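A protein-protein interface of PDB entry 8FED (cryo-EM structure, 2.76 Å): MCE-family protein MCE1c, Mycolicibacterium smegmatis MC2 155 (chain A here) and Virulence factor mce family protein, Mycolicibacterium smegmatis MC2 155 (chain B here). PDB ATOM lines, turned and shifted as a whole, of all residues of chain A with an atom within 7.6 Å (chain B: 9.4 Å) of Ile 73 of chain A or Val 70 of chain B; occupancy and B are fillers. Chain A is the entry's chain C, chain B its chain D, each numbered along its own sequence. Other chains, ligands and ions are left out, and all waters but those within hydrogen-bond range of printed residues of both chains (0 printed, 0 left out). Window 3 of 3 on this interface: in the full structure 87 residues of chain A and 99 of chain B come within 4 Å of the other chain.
Among the printed residues, pairs that only touch across the chains: Asp 76 of chain A with Pro 121 of chain B, Thr 49 of chain A with Gly 69 of chain B, Ile 73 of chain A with Ile 67 of chain B, Ile 73 of chain A with Val 70 of chain B, Val 78 of chain A with Met 68 of chain B, Asp 48 of chain A with Met 68 of chain B, Ile 73 of chain A with Met 68 of chain B, Lys 77 of chain A with Met 68 of chain B, Asp 48 of chain A with Gln 117 of chain B, Gly 75 of chain A with Met 68 of chain B and Thr 49 of chain A with Val 70 of chain B.
The backbone NH of Thr 49 of chain A sits close to the backbone carbonyl oxygen of Met 68 of chain B (3.4 Å). SD of Met 68 of chain B lies close to O of Asp 76 of chain A (3.3 Å).
OD1 of Asp 48 of chain A is in hydrogen-bond range of N of Gly 50 of chain A (2.5 Å).
Met 71 of chain A touches none of the printed residues of chain B. Ile 73 of chain A touches just these residues of chain B: Ile 67, Met 68 and Val 70. Gly 75 of chain A touches one residue of chain B. Of the printed residues of chain B, Lys 77 of chain A touches Met 68. Of the printed residues of chain A, Met 68 of chain B touches Asp 48, Thr 49, Ile 73, Gly 75, Asp 76, Lys 77 and Val 78. Printed residues of chain A within 4 Å of Gly 69 of chain B: Thr 49 (3.3 Å). Tyr 95 of chain B touches none of the printed residues of chain A. Printed residues of chain A within 4 Å of Gln 117 of chain B: Asp 48 (3.8 Å). Of the printed residues of chain A, Pro 121 of chain B touches Asp 76 (3.2 Å). The nearest residue of chain B that does not touch Ile 73 of chain A is Val 72 of chain B (4.1 Å). The nearest residue of chain A that does not touch Val 70 of chain B is Val 78 of chain A (4.4 Å). The nearest printed residue of chain A that does not touch Gln 117 of chain B is Thr 49 of chain A (6.9 Å).
Of the 24 printed residues of chain B, 6 touch a printed residue of chain A. Of the 14 printed residues of chain A, 7 touch a printed residue of chain B. Hydrophobic or aromatic side chains of chain A within 4 Å of the printed part of chain B: Ile 73 and Val 78. Among the printed residues, no Asp or Glu carboxylate lies within 4 Å of a Lys or Arg side-chain nitrogen of the other chain.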
ATOM      1  N   ASP A  48     -10.362  18.754  29.820  1.00  0.00           N
ATOM      2  CA  ASP A  48      -9.933  19.549  28.679  1.00  0.00           C
ATOM      3  C   ASP A  48      -8.603  20.198  29.030  1.00  0.00           C
ATOM      4  O   ASP A  48      -8.336  20.501  30.196  1.00  0.00           O
ATOM      5  CB  ASP A  48     -10.989  20.605  28.317  1.00  0.00           C
ATOM      6  CG  ASP A  48     -10.680  21.345  27.019  1.00  0.00           C
ATOM      7  OD1 ASP A  48      -9.568  21.893  26.865  1.00  0.00           O
ATOM      8  OD2 ASP A  48     -11.568  21.383  26.142  1.00  0.00           O
ATOM      9  N   THR A  49      -7.769  20.404  28.007  1.00  0.00           N
ATOM     10  CA  THR A  49      -6.503  21.096  28.222  1.00  0.00           C
ATOM     11  C   THR A  49      -6.732  22.568  28.540  1.00  0.00           C
ATOM     12  O   THR A  49      -6.011  23.153  29.354  1.00  0.00           O
ATOM     13  CB  THR A  49      -5.599  20.952  27.000  1.00  0.00           C
ATOM     14  OG1 THR A  49      -6.149  21.699  25.909  1.00  0.00           O
ATOM     15  CG2 THR A  49      -5.480  19.496  26.598  1.00  0.00           C
ATOM     16  N   GLY A  50      -7.728  23.178  27.908  1.00  0.00           N
ATOM     17  CA  GLY A  50      -8.029  24.579  28.145  1.00  0.00           C
ATOM     18  C   GLY A  50      -6.950  25.542  27.702  1.00  0.00           C
ATOM     19  O   GLY A  50      -6.638  26.492  28.431  1.00  0.00           O
ATOM     20  N   LEU A  52      -3.805  24.894  27.435  1.00  0.00           N
ATOM     21  CA  LEU A  52      -2.521  24.592  28.050  1.00  0.00           C
ATOM     22  C   LEU A  52      -1.520  24.134  26.995  1.00  0.00           C
ATOM     23  O   LEU A  52      -1.857  23.371  26.086  1.00  0.00           O
ATOM     24  CB  LEU A  52      -2.694  23.516  29.120  1.00  0.00           C
ATOM     25  CG  LEU A  52      -1.597  23.378  30.172  1.00  0.00           C
ATOM     26  CD1 LEU A  52      -1.483  24.651  30.987  1.00  0.00           C
ATOM     27  CD2 LEU A  52      -1.885  22.195  31.071  1.00  0.00           C
ATOM     28  N   MET A  71       0.998  16.105  26.816  1.00  0.00           N
ATOM     29  CA  MET A  71      -0.462  16.094  26.776  1.00  0.00           C
ATOM     30  C   MET A  71      -0.905  15.052  25.761  1.00  0.00           C
ATOM     31  O   MET A  71      -0.522  15.129  24.590  1.00  0.00           O
ATOM     32  CB  MET A  71      -1.027  17.469  26.406  1.00  0.00           C
ATOM     33  CG  MET A  71      -0.645  18.591  27.354  1.00  0.00           C
ATOM     34  SD  MET A  71      -1.401  20.163  26.905  1.00  0.00           S
ATOM     35  CE  MET A  71      -0.852  20.324  25.210  1.00  0.00           C
ATOM     36  N   GLU A  72      -1.708  14.085  26.199  1.00  0.00           N
ATOM     37  CA  GLU A  72      -2.201  13.031  25.325  1.00  0.00           C
ATOM     38  C   GLU A  72      -3.694  12.839  25.544  1.00  0.00           C
ATOM     39  O   GLU A  72      -4.240  13.204  26.585  1.00  0.00           O
ATOM     40  CB  GLU A  72      -1.464  11.704  25.564  1.00  0.00           C
ATOM     41  CG  GLU A  72      -0.001  11.705  25.147  1.00  0.00           C
ATOM     42  CD  GLU A  72       0.187  11.688  23.640  1.00  0.00           C
ATOM     43  OE1 GLU A  72      -0.776  11.355  22.917  1.00  0.00           O
ATOM     44  OE2 GLU A  72       1.303  12.008  23.177  1.00  0.00           O
ATOM     45  N   ILE A  73      -4.356  12.268  24.543  1.00  0.00           N
ATOM     46  CA  ILE A  73      -5.777  11.946  24.616  1.00  0.00           C
ATOM     47  C   ILE A  73      -5.913  10.482  25.009  1.00  0.00           C
ATOM     48  O   ILE A  73      -5.446   9.593  24.287  1.00  0.00           O
ATOM     49  CB  ILE A  73      -6.489  12.223  23.283  1.00  0.00           C
ATOM     50  CG1 ILE A  73      -6.570  13.726  23.015  1.00  0.00           C
ATOM     51  CG2 ILE A  73      -7.876  11.602  23.279  1.00  0.00           C
ATOM     52  CD1 ILE A  73      -7.214  14.065  21.693  1.00  0.00           C
ATOM     53  N   ASP A  74      -6.549  10.224  26.150  1.00  0.00           N
ATOM     54  CA  ASP A  74      -6.756   8.867  26.647  1.00  0.00           C
ATOM     55  C   ASP A  74      -8.258   8.669  26.820  1.00  0.00           C
ATOM     56  O   ASP A  74      -8.829   9.055  27.846  1.00  0.00           O
ATOM     57  CB  ASP A  74      -6.004   8.638  27.955  1.00  0.00           C
ATOM     58  CG  ASP A  74      -6.105   7.207  28.443  1.00  0.00           C
ATOM     59  OD1 ASP A  74      -5.513   6.314  27.801  1.00  0.00           O
ATOM     60  OD2 ASP A  74      -6.776   6.973  29.471  1.00  0.00           O
ATOM     61  N   GLY A  75      -8.884   8.070  25.814  1.00  0.00           N
ATOM     62  CA  GLY A  75     -10.315   7.810  25.854  1.00  0.00           C
ATOM     63  C   GLY A  75     -11.121   9.083  26.014  1.00  0.00           C
ATOM     64  O   GLY A  75     -11.070   9.993  25.178  1.00  0.00           O
ATOM     65  N   ASP A  76     -11.880   9.152  27.105  1.00  0.00           N
ATOM     66  CA  ASP A  76     -12.713  10.307  27.404  1.00  0.00           C
ATOM     67  C   ASP A  76     -11.935  11.455  28.037  1.00  0.00           C
ATOM     68  O   ASP A  76     -12.474  12.562  28.147  1.00  0.00           O
ATOM     69  CB  ASP A  76     -13.854   9.874  28.332  1.00  0.00           C
ATOM     70  CG  ASP A  76     -14.975  10.892  28.410  1.00  0.00           C
ATOM     71  OD1 ASP A  76     -15.038  11.784  27.540  1.00  0.00           O
ATOM     72  OD2 ASP A  76     -15.796  10.799  29.346  1.00  0.00           O
ATOM     73  N   LYS A  77     -10.688  11.234  28.437  1.00  0.00           N
ATOM     74  CA  LYS A  77      -9.943  12.206  29.222  1.00  0.00           C
ATOM     75  C   LYS A  77      -8.694  12.661  28.480  1.00  0.00           C
ATOM     76  O   LYS A  77      -8.330  12.130  27.427  1.00  0.00           O
ATOM     77  CB  LYS A  77      -9.557  11.618  30.585  1.00  0.00           C
ATOM     78  CG  LYS A  77     -10.726  11.041  31.360  1.00  0.00           C
ATOM     79  CD  LYS A  77     -10.249  10.111  32.456  1.00  0.00           C
ATOM     80  CE  LYS A  77      -9.478   8.937  31.875  1.00  0.00           C
ATOM     81  NZ  LYS A  77     -10.329   8.100  30.984  1.00  0.00           N
ATOM     82  N   VAL A  78      -8.033  13.662  29.052  1.00  0.00           N
ATOM     83  CA  VAL A  78      -6.726  14.114  28.598  1.00  0.00           C
ATOM     84  C   VAL A  78      -5.732  13.843  29.716  1.00  0.00           C
ATOM     85  O   VAL A  78      -5.913  14.320  30.842  1.00  0.00           O
ATOM     86  CB  VAL A  78      -6.731  15.602  28.221  1.00  0.00           C
ATOM     87  CG1 VAL A  78      -5.320  16.082  27.949  1.00  0.00           C
ATOM     88  CG2 VAL A  78      -7.612  15.834  27.012  1.00  0.00           C
ATOM     89  N   VAL A  79      -4.694  13.076  29.411  1.00  0.00           N
ATOM     90  CA  VAL A  79      -3.634  12.790  30.369  1.00  0.00           C
ATOM     91  C   VAL A  79      -2.539  13.828  30.181  1.00  0.00           C
ATOM     92  O   VAL A  79      -1.920  13.907  29.114  1.00  0.00           O
ATOM     93  CB  VAL A  79      -3.088  11.366  30.195  1.00  0.00           C
ATOM     94  CG1 VAL A  79      -1.863  11.165  31.067  1.00  0.00           C
ATOM     95  CG2 VAL A  79      -4.156  10.355  30.553  1.00  0.00           C
ATOM     96  N   ILE A  80      -2.309  14.631  31.213  1.00  0.00           N
ATOM     97  CA  ILE A  80      -1.286  15.667  31.202  1.00  0.00           C
ATOM     98  C   ILE A  80      -0.198  15.251  32.179  1.00  0.00           C
ATOM     99  O   ILE A  80      -0.459  15.075  33.376  1.00  0.00           O
ATOM    100  CB  ILE A  80      -1.867  17.042  31.566  1.00  0.00           C
ATOM    101  CG1 ILE A  80      -2.931  17.451  30.546  1.00  0.00           C
ATOM    102  CG2 ILE A  80      -0.767  18.080  31.634  1.00  0.00           C
ATOM    103  CD1 ILE A  80      -3.489  18.836  30.766  1.00  0.00           C
ATOM    104  N   LYS B  64      -5.556  24.550  12.923  1.00  0.00           N
ATOM    105  CA  LYS B  64      -5.571  23.265  13.603  1.00  0.00           C
ATOM    106  C   LYS B  64      -6.991  22.831  13.945  1.00  0.00           C
ATOM    107  O   LYS B  64      -7.883  23.652  14.167  1.00  0.00           O
ATOM    108  CB  LYS B  64      -4.727  23.329  14.875  1.00  0.00           C
ATOM    109  CG  LYS B  64      -3.329  23.883  14.661  1.00  0.00           C
ATOM    110  CD  LYS B  64      -2.588  23.114  13.581  1.00  0.00           C
ATOM    111  CE  LYS B  64      -1.221  23.719  13.317  1.00  0.00           C
ATOM    112  NZ  LYS B  64      -0.500  23.002  12.230  1.00  0.00           N
ATOM    113  N   VAL B  65      -7.190  21.518  13.979  1.00  0.00           N
ATOM    114  CA  VAL B  65      -8.430  20.901  14.436  1.00  0.00           C
ATOM    115  C   VAL B  65      -8.135  20.214  15.759  1.00  0.00           C
ATOM    116  O   VAL B  65      -7.151  19.475  15.873  1.00  0.00           O
ATOM    117  CB  VAL B  65      -8.985  19.910  13.397  1.00  0.00           C
ATOM    118  CG1 VAL B  65     -10.092  19.063  13.999  1.00  0.00           C
ATOM    119  CG2 VAL B  65      -9.494  20.657  12.179  1.00  0.00           C
ATOM    120  N   LEU B  66      -8.968  20.475  16.762  1.00  0.00           N
ATOM    121  CA  LEU B  66      -8.712  20.025  18.120  1.00  0.00           C
ATOM    122  C   LEU B  66      -9.768  19.030  18.577  1.00  0.00           C
ATOM    123  O   LEU B  66     -10.932  19.100  18.178  1.00  0.00           O
ATOM    124  CB  LEU B  66      -8.682  21.199  19.105  1.00  0.00           C
ATOM    125  CG  LEU B  66      -7.762  22.384  18.824  1.00  0.00           C
ATOM    126  CD1 LEU B  66      -7.771  23.326  20.008  1.00  0.00           C
ATOM    127  CD2 LEU B  66      -6.357  21.919  18.526  1.00  0.00           C
ATOM    128  N   ILE B  67      -9.335  18.090  19.409  1.00  0.00           N
ATOM    129  CA  ILE B  67     -10.220  17.258  20.212  1.00  0.00           C
ATOM    130  C   ILE B  67      -9.776  17.424  21.655  1.00  0.00           C
ATOM    131  O   ILE B  67      -8.632  17.095  21.996  1.00  0.00           O
ATOM    132  CB  ILE B  67     -10.184  15.783  19.787  1.00  0.00           C
ATOM    133  CG1 ILE B  67     -10.750  15.621  18.376  1.00  0.00           C
ATOM    134  CG2 ILE B  67     -10.965  14.930  20.771  1.00  0.00           C
ATOM    135  CD1 ILE B  67     -10.750  14.194  17.880  1.00  0.00           C
ATOM    136  N   MET B  68     -10.666  17.965  22.492  1.00  0.00           N
ATOM    137  CA  MET B  68     -10.370  18.259  23.896  1.00  0.00           C
ATOM    138  C   MET B  68      -9.111  19.110  24.035  1.00  0.00           C
ATOM    139  O   MET B  68      -8.342  18.962  24.987  1.00  0.00           O
ATOM    140  CB  MET B  68     -10.253  16.976  24.720  1.00  0.00           C
ATOM    141  CG  MET B  68     -11.578  16.277  24.955  1.00  0.00           C
ATOM    142  SD  MET B  68     -11.413  14.772  25.930  1.00  0.00           S
ATOM    143  CE  MET B  68     -10.451  13.759  24.815  1.00  0.00           C
ATOM    144  N   GLY B  69      -8.894  20.011  23.078  1.00  0.00           N
ATOM    145  CA  GLY B  69      -7.758  20.903  23.094  1.00  0.00           C
ATOM    146  C   GLY B  69      -6.479  20.340  22.513  1.00  0.00           C
ATOM    147  O   GLY B  69      -5.471  21.057  22.477  1.00  0.00           O
ATOM    148  N   VAL B  70      -6.481  19.091  22.054  1.00  0.00           N
ATOM    149  CA  VAL B  70      -5.289  18.450  21.509  1.00  0.00           C
ATOM    150  C   VAL B  70      -5.411  18.399  19.994  1.00  0.00           C
ATOM    151  O   VAL B  70      -6.447  17.980  19.465  1.00  0.00           O
ATOM    152  CB  VAL B  70      -5.098  17.041  22.096  1.00  0.00           C
ATOM    153  CG1 VAL B  70      -3.821  16.413  21.568  1.00  0.00           C
ATOM    154  CG2 VAL B  70      -5.081  17.101  23.613  1.00  0.00           C
ATOM    155  N   ARG B  71      -4.366  18.848  19.297  1.00  0.00           N
ATOM    156  CA  ARG B  71      -4.372  18.850  17.838  1.00  0.00           C
ATOM    157  C   ARG B  71      -4.475  17.430  17.297  1.00  0.00           C
ATOM    158  O   ARG B  71      -3.747  16.534  17.732  1.00  0.00           O
ATOM    159  CB  ARG B  71      -3.105  19.518  17.306  1.00  0.00           C
ATOM    160  CG  ARG B  71      -2.919  20.961  17.737  1.00  0.00           C
ATOM    161  CD  ARG B  71      -1.637  21.540  17.162  1.00  0.00           C
ATOM    162  NE  ARG B  71      -1.459  22.944  17.513  1.00  0.00           N
ATOM    163  CZ  ARG B  71      -0.455  23.700  17.090  1.00  0.00           C
ATOM    164  NH1 ARG B  71       0.488  23.217  16.299  1.00  0.00           N
ATOM    165  NH2 ARG B  71      -0.395  24.973  17.471  1.00  0.00           N
ATOM    166  N   VAL B  72      -5.383  17.226  16.344  1.00  0.00           N
ATOM    167  CA  VAL B  72      -5.584  15.912  15.743  1.00  0.00           C
ATOM    168  C   VAL B  72      -5.620  16.031  14.225  1.00  0.00           C
ATOM    169  O   VAL B  72      -5.667  15.021  13.516  1.00  0.00           O
ATOM    170  CB  VAL B  72      -6.876  15.252  16.258  1.00  0.00           C
ATOM    171  CG1 VAL B  72      -6.776  14.958  17.747  1.00  0.00           C
ATOM    172  CG2 VAL B  72      -8.070  16.139  15.961  1.00  0.00           C
ATOM    173  N   GLY B  73      -5.598  17.255  13.715  1.00  0.00           N
ATOM    174  CA  GLY B  73      -5.682  17.445  12.282  1.00  0.00           C
ATOM    175  C   GLY B  73      -5.604  18.906  11.911  1.00  0.00           C
ATOM    176  O   GLY B  73      -5.114  19.733  12.681  1.00  0.00           O
ATOM    177  N   SER B  74      -6.093  19.216  10.713  1.00  0.00           N
ATOM    178  CA  SER B  74      -6.032  20.572  10.185  1.00  0.00           C
ATOM    179  C   SER B  74      -7.255  20.810   9.307  1.00  0.00           C
ATOM    180  O   SER B  74      -8.153  19.968   9.219  1.00  0.00           O
ATOM    181  CB  SER B  74      -4.720  20.791   9.425  1.00  0.00           C
ATOM    182  OG  SER B  74      -4.641  22.109   8.918  1.00  0.00           O
ATOM    183  N   PHE B  91      -8.914  15.149  10.174  1.00  0.00           N
ATOM    184  CA  PHE B  91      -8.276  14.781  11.429  1.00  0.00           C
ATOM    185  C   PHE B  91      -7.668  13.393  11.293  1.00  0.00           C
ATOM    186  O   PHE B  91      -8.160  12.557  10.531  1.00  0.00           O
ATOM    187  CB  PHE B  91      -9.256  14.824  12.613  1.00  0.00           C
ATOM    188  CG  PHE B  91     -10.473  13.962  12.435  1.00  0.00           C
ATOM    189  CD1 PHE B  91     -10.473  12.641  12.848  1.00  0.00           C
ATOM    190  CD2 PHE B  91     -11.627  14.483  11.877  1.00  0.00           C
ATOM    191  CE1 PHE B  91     -11.591  11.850  12.686  1.00  0.00           C
ATOM    192  CE2 PHE B  91     -12.749  13.699  11.718  1.00  0.00           C
ATOM    193  CZ  PHE B  91     -12.732  12.381  12.123  1.00  0.00           C
ATOM    194  N   ASN B  92      -6.597  13.160  12.051  1.00  0.00           N
ATOM    195  CA  ASN B  92      -5.847  11.913  11.955  1.00  0.00           C
ATOM    196  C   ASN B  92      -6.749  10.721  12.247  1.00  0.00           C
ATOM    197  O   ASN B  92      -7.574  10.753  13.163  1.00  0.00           O
ATOM    198  CB  ASN B  92      -4.663  11.937  12.924  1.00  0.00           C
ATOM    199  CG  ASN B  92      -3.641  10.845  12.641  1.00  0.00           C
ATOM    200  OD1 ASN B  92      -3.983   9.732  12.242  1.00  0.00           O
ATOM    201  ND2 ASN B  92      -2.370  11.168  12.847  1.00  0.00           N
ATOM    202  N   LYS B  94      -6.128   8.002  13.595  1.00  0.00           N
ATOM    203  CA  LYS B  94      -5.900   7.340  14.876  1.00  0.00           C
ATOM    204  C   LYS B  94      -7.022   7.640  15.862  1.00  0.00           C
ATOM    205  O   LYS B  94      -7.467   6.753  16.599  1.00  0.00           O
ATOM    206  CB  LYS B  94      -4.555   7.773  15.458  1.00  0.00           C
ATOM    207  CG  LYS B  94      -3.357   7.440  14.590  1.00  0.00           C
ATOM    208  CD  LYS B  94      -2.100   8.119  15.112  1.00  0.00           C
ATOM    209  CE  LYS B  94      -1.895   7.846  16.593  1.00  0.00           C
ATOM    210  NZ  LYS B  94      -0.696   8.546  17.126  1.00  0.00           N
ATOM    211  N   TYR B  95      -7.487   8.885  15.891  1.00  0.00           N
ATOM    212  CA  TYR B  95      -8.518   9.310  16.825  1.00  0.00           C
ATOM    213  C   TYR B  95      -9.894   9.138  16.195  1.00  0.00           C
ATOM    214  O   TYR B  95     -10.108   9.521  15.041  1.00  0.00           O
ATOM    215  CB  TYR B  95      -8.300  10.767  17.235  1.00  0.00           C
ATOM    216  CG  TYR B  95      -6.868  11.092  17.592  1.00  0.00           C
ATOM    217  CD1 TYR B  95      -6.375  10.839  18.864  1.00  0.00           C
ATOM    218  CD2 TYR B  95      -6.009  11.652  16.656  1.00  0.00           C
ATOM    219  CE1 TYR B  95      -5.067  11.134  19.195  1.00  0.00           C
ATOM    220  CE2 TYR B  95      -4.700  11.951  16.977  1.00  0.00           C
ATOM    221  CZ  TYR B  95      -4.235  11.691  18.247  1.00  0.00           C
ATOM    222  OH  TYR B  95      -2.932  11.987  18.571  1.00  0.00           O
ATOM    223  N   LYS B  96     -10.818   8.564  16.955  1.00  0.00           N
ATOM    224  CA  LYS B  96     -12.180   8.339  16.496  1.00  0.00           C
ATOM    225  C   LYS B  96     -13.105   9.413  17.054  1.00  0.00           C
ATOM    226  O   LYS B  96     -12.924   9.896  18.175  1.00  0.00           O
ATOM    227  CB  LYS B  96     -12.672   6.952  16.911  1.00  0.00           C
ATOM    228  CG  LYS B  96     -12.031   5.817  16.129  1.00  0.00           C
ATOM    229  CD  LYS B  96     -12.421   4.461  16.692  1.00  0.00           C
ATOM    230  CE  LYS B  96     -11.841   4.256  18.082  1.00  0.00           C
ATOM    231  NZ  LYS B  96     -12.183   2.916  18.634  1.00  0.00           N
ATOM    232  N   VAL B  97     -14.093   9.794  16.250  1.00  0.00           N
ATOM    233  CA  VAL B  97     -14.993  10.898  16.572  1.00  0.00           C
ATOM    234  C   VAL B  97     -16.429  10.396  16.465  1.00  0.00           C
ATOM    235  O   VAL B  97     -16.755   9.680  15.508  1.00  0.00           O
ATOM    236  CB  VAL B  97     -14.737  12.095  15.639  1.00  0.00           C
ATOM    237  CG1 VAL B  97     -15.634  13.266  15.977  1.00  0.00           C
ATOM    238  CG2 VAL B  97     -13.282  12.519  15.714  1.00  0.00           C
ATOM    239  N   LEU B 106     -13.615  27.840  17.667  1.00  0.00           N
ATOM    240  CA  LEU B 106     -13.192  28.415  18.934  1.00  0.00           C
ATOM    241  C   LEU B 106     -12.108  29.456  18.708  1.00  0.00           C
ATOM    242  O   LEU B 106     -11.245  29.294  17.837  1.00  0.00           O
ATOM    243  CB  LEU B 106     -12.678  27.336  19.892  1.00  0.00           C
ATOM    244  CG  LEU B 106     -13.680  26.260  20.308  1.00  0.00           C
ATOM    245  CD1 LEU B 106     -13.020  25.256  21.228  1.00  0.00           C
ATOM    246  CD2 LEU B 106     -14.890  26.887  20.980  1.00  0.00           C
ATOM    247  N   VAL B 115      -9.683  27.756  15.882  1.00  0.00           N
ATOM    248  CA  VAL B 115      -9.607  26.329  15.609  1.00  0.00           C
ATOM    249  C   VAL B 115     -11.017  25.777  15.461  1.00  0.00           C
ATOM    250  O   VAL B 115     -12.005  26.451  15.743  1.00  0.00           O
ATOM    251  CB  VAL B 115      -8.852  25.568  16.716  1.00  0.00           C
ATOM    252  CG1 VAL B 115      -7.416  26.048  16.810  1.00  0.00           C
ATOM    253  CG2 VAL B 115      -9.561  25.756  18.042  1.00  0.00           C
ATOM    254  N   ILE B 116     -11.099  24.532  15.004  1.00  0.00           N
ATOM    255  CA  ILE B 116     -12.351  23.786  14.957  1.00  0.00           C
ATOM    256  C   ILE B 116     -12.213  22.609  15.907  1.00  0.00           C
ATOM    257  O   ILE B 116     -11.333  21.759  15.724  1.00  0.00           O
ATOM    258  CB  ILE B 116     -12.688  23.308  13.536  1.00  0.00           C
ATOM    259  CG1 ILE B 116     -13.120  24.485  12.664  1.00  0.00           C
ATOM    260  CG2 ILE B 116     -13.773  22.243  13.574  1.00  0.00           C
ATOM    261  CD1 ILE B 116     -13.596  24.079  11.290  1.00  0.00           C
ATOM    262  N   GLN B 117     -13.075  22.553  16.916  1.00  0.00           N
ATOM    263  CA  GLN B 117     -13.049  21.484  17.901  1.00  0.00           C
ATOM    264  C   GLN B 117     -14.302  20.635  17.762  1.00  0.00           C
ATOM    265  O   GLN B 117     -15.415  21.166  17.695  1.00  0.00           O
ATOM    266  CB  GLN B 117     -12.939  22.038  19.323  1.00  0.00           C
ATOM    267  CG  GLN B 117     -12.984  20.961  20.394  1.00  0.00           C
ATOM    268  CD  GLN B 117     -12.589  21.472  21.762  1.00  0.00           C
ATOM    269  OE1 GLN B 117     -11.734  22.346  21.886  1.00  0.00           O
ATOM    270  NE2 GLN B 117     -13.212  20.928  22.798  1.00  0.00           N
ATOM    271  N   LEU B 118     -14.112  19.321  17.699  1.00  0.00           N
ATOM    272  CA  LEU B 118     -15.215  18.368  17.750  1.00  0.00           C
ATOM    273  C   LEU B 118     -15.609  18.204  19.212  1.00  0.00           C
ATOM    274  O   LEU B 118     -15.006  17.418  19.946  1.00  0.00           O
ATOM    275  CB  LEU B 118     -14.800  17.051  17.107  1.00  0.00           C
ATOM    276  CG  LEU B 118     -14.308  17.259  15.672  1.00  0.00           C
ATOM    277  CD1 LEU B 118     -13.441  16.109  15.210  1.00  0.00           C
ATOM    278  CD2 LEU B 118     -15.483  17.454  14.729  1.00  0.00           C
ATOM    279  N   PRO B 121     -16.533  14.455  23.201  1.00  0.00           N
ATOM    280  CA  PRO B 121     -15.491  13.426  23.124  1.00  0.00           C
ATOM    281  C   PRO B 121     -16.081  12.051  22.859  1.00  0.00           C
ATOM    282  O   PRO B 121     -17.215  11.749  23.237  1.00  0.00           O
ATOM    283  CB  PRO B 121     -14.827  13.492  24.503  1.00  0.00           C
ATOM    284  CG  PRO B 121     -15.889  14.030  25.397  1.00  0.00           C
ATOM    285  CD  PRO B 121     -16.693  14.983  24.567  1.00  0.00           C
ATOM    286  N   TYR B 122     -15.287  11.212  22.202  1.00  0.00           N
ATOM    287  CA  TYR B 122     -15.738   9.883  21.806  1.00  0.00           C
ATOM    288  C   TYR B 122     -15.697   8.932  22.994  1.00  0.00           C
ATOM    289  O   TYR B 122     -14.678   8.828  23.684  1.00  0.00           O
ATOM    290  CB  TYR B 122     -14.873   9.347  20.668  1.00  0.00           C
ATOM    291  CG  TYR B 122     -15.283   7.983  20.166  1.00  0.00           C
ATOM    292  CD1 TYR B 122     -16.360   7.835  19.305  1.00  0.00           C
ATOM    293  CD2 TYR B 122     -14.584   6.844  20.542  1.00  0.00           C
ATOM    294  CE1 TYR B 122     -16.737   6.590  18.839  1.00  0.00           C
ATOM    295  CE2 TYR B 122     -14.953   5.595  20.083  1.00  0.00           C
ATOM    296  CZ  TYR B 122     -16.029   5.473  19.231  1.00  0.00           C
ATOM    297  OH  TYR B 122     -16.400   4.232  18.768  1.00  0.00           O
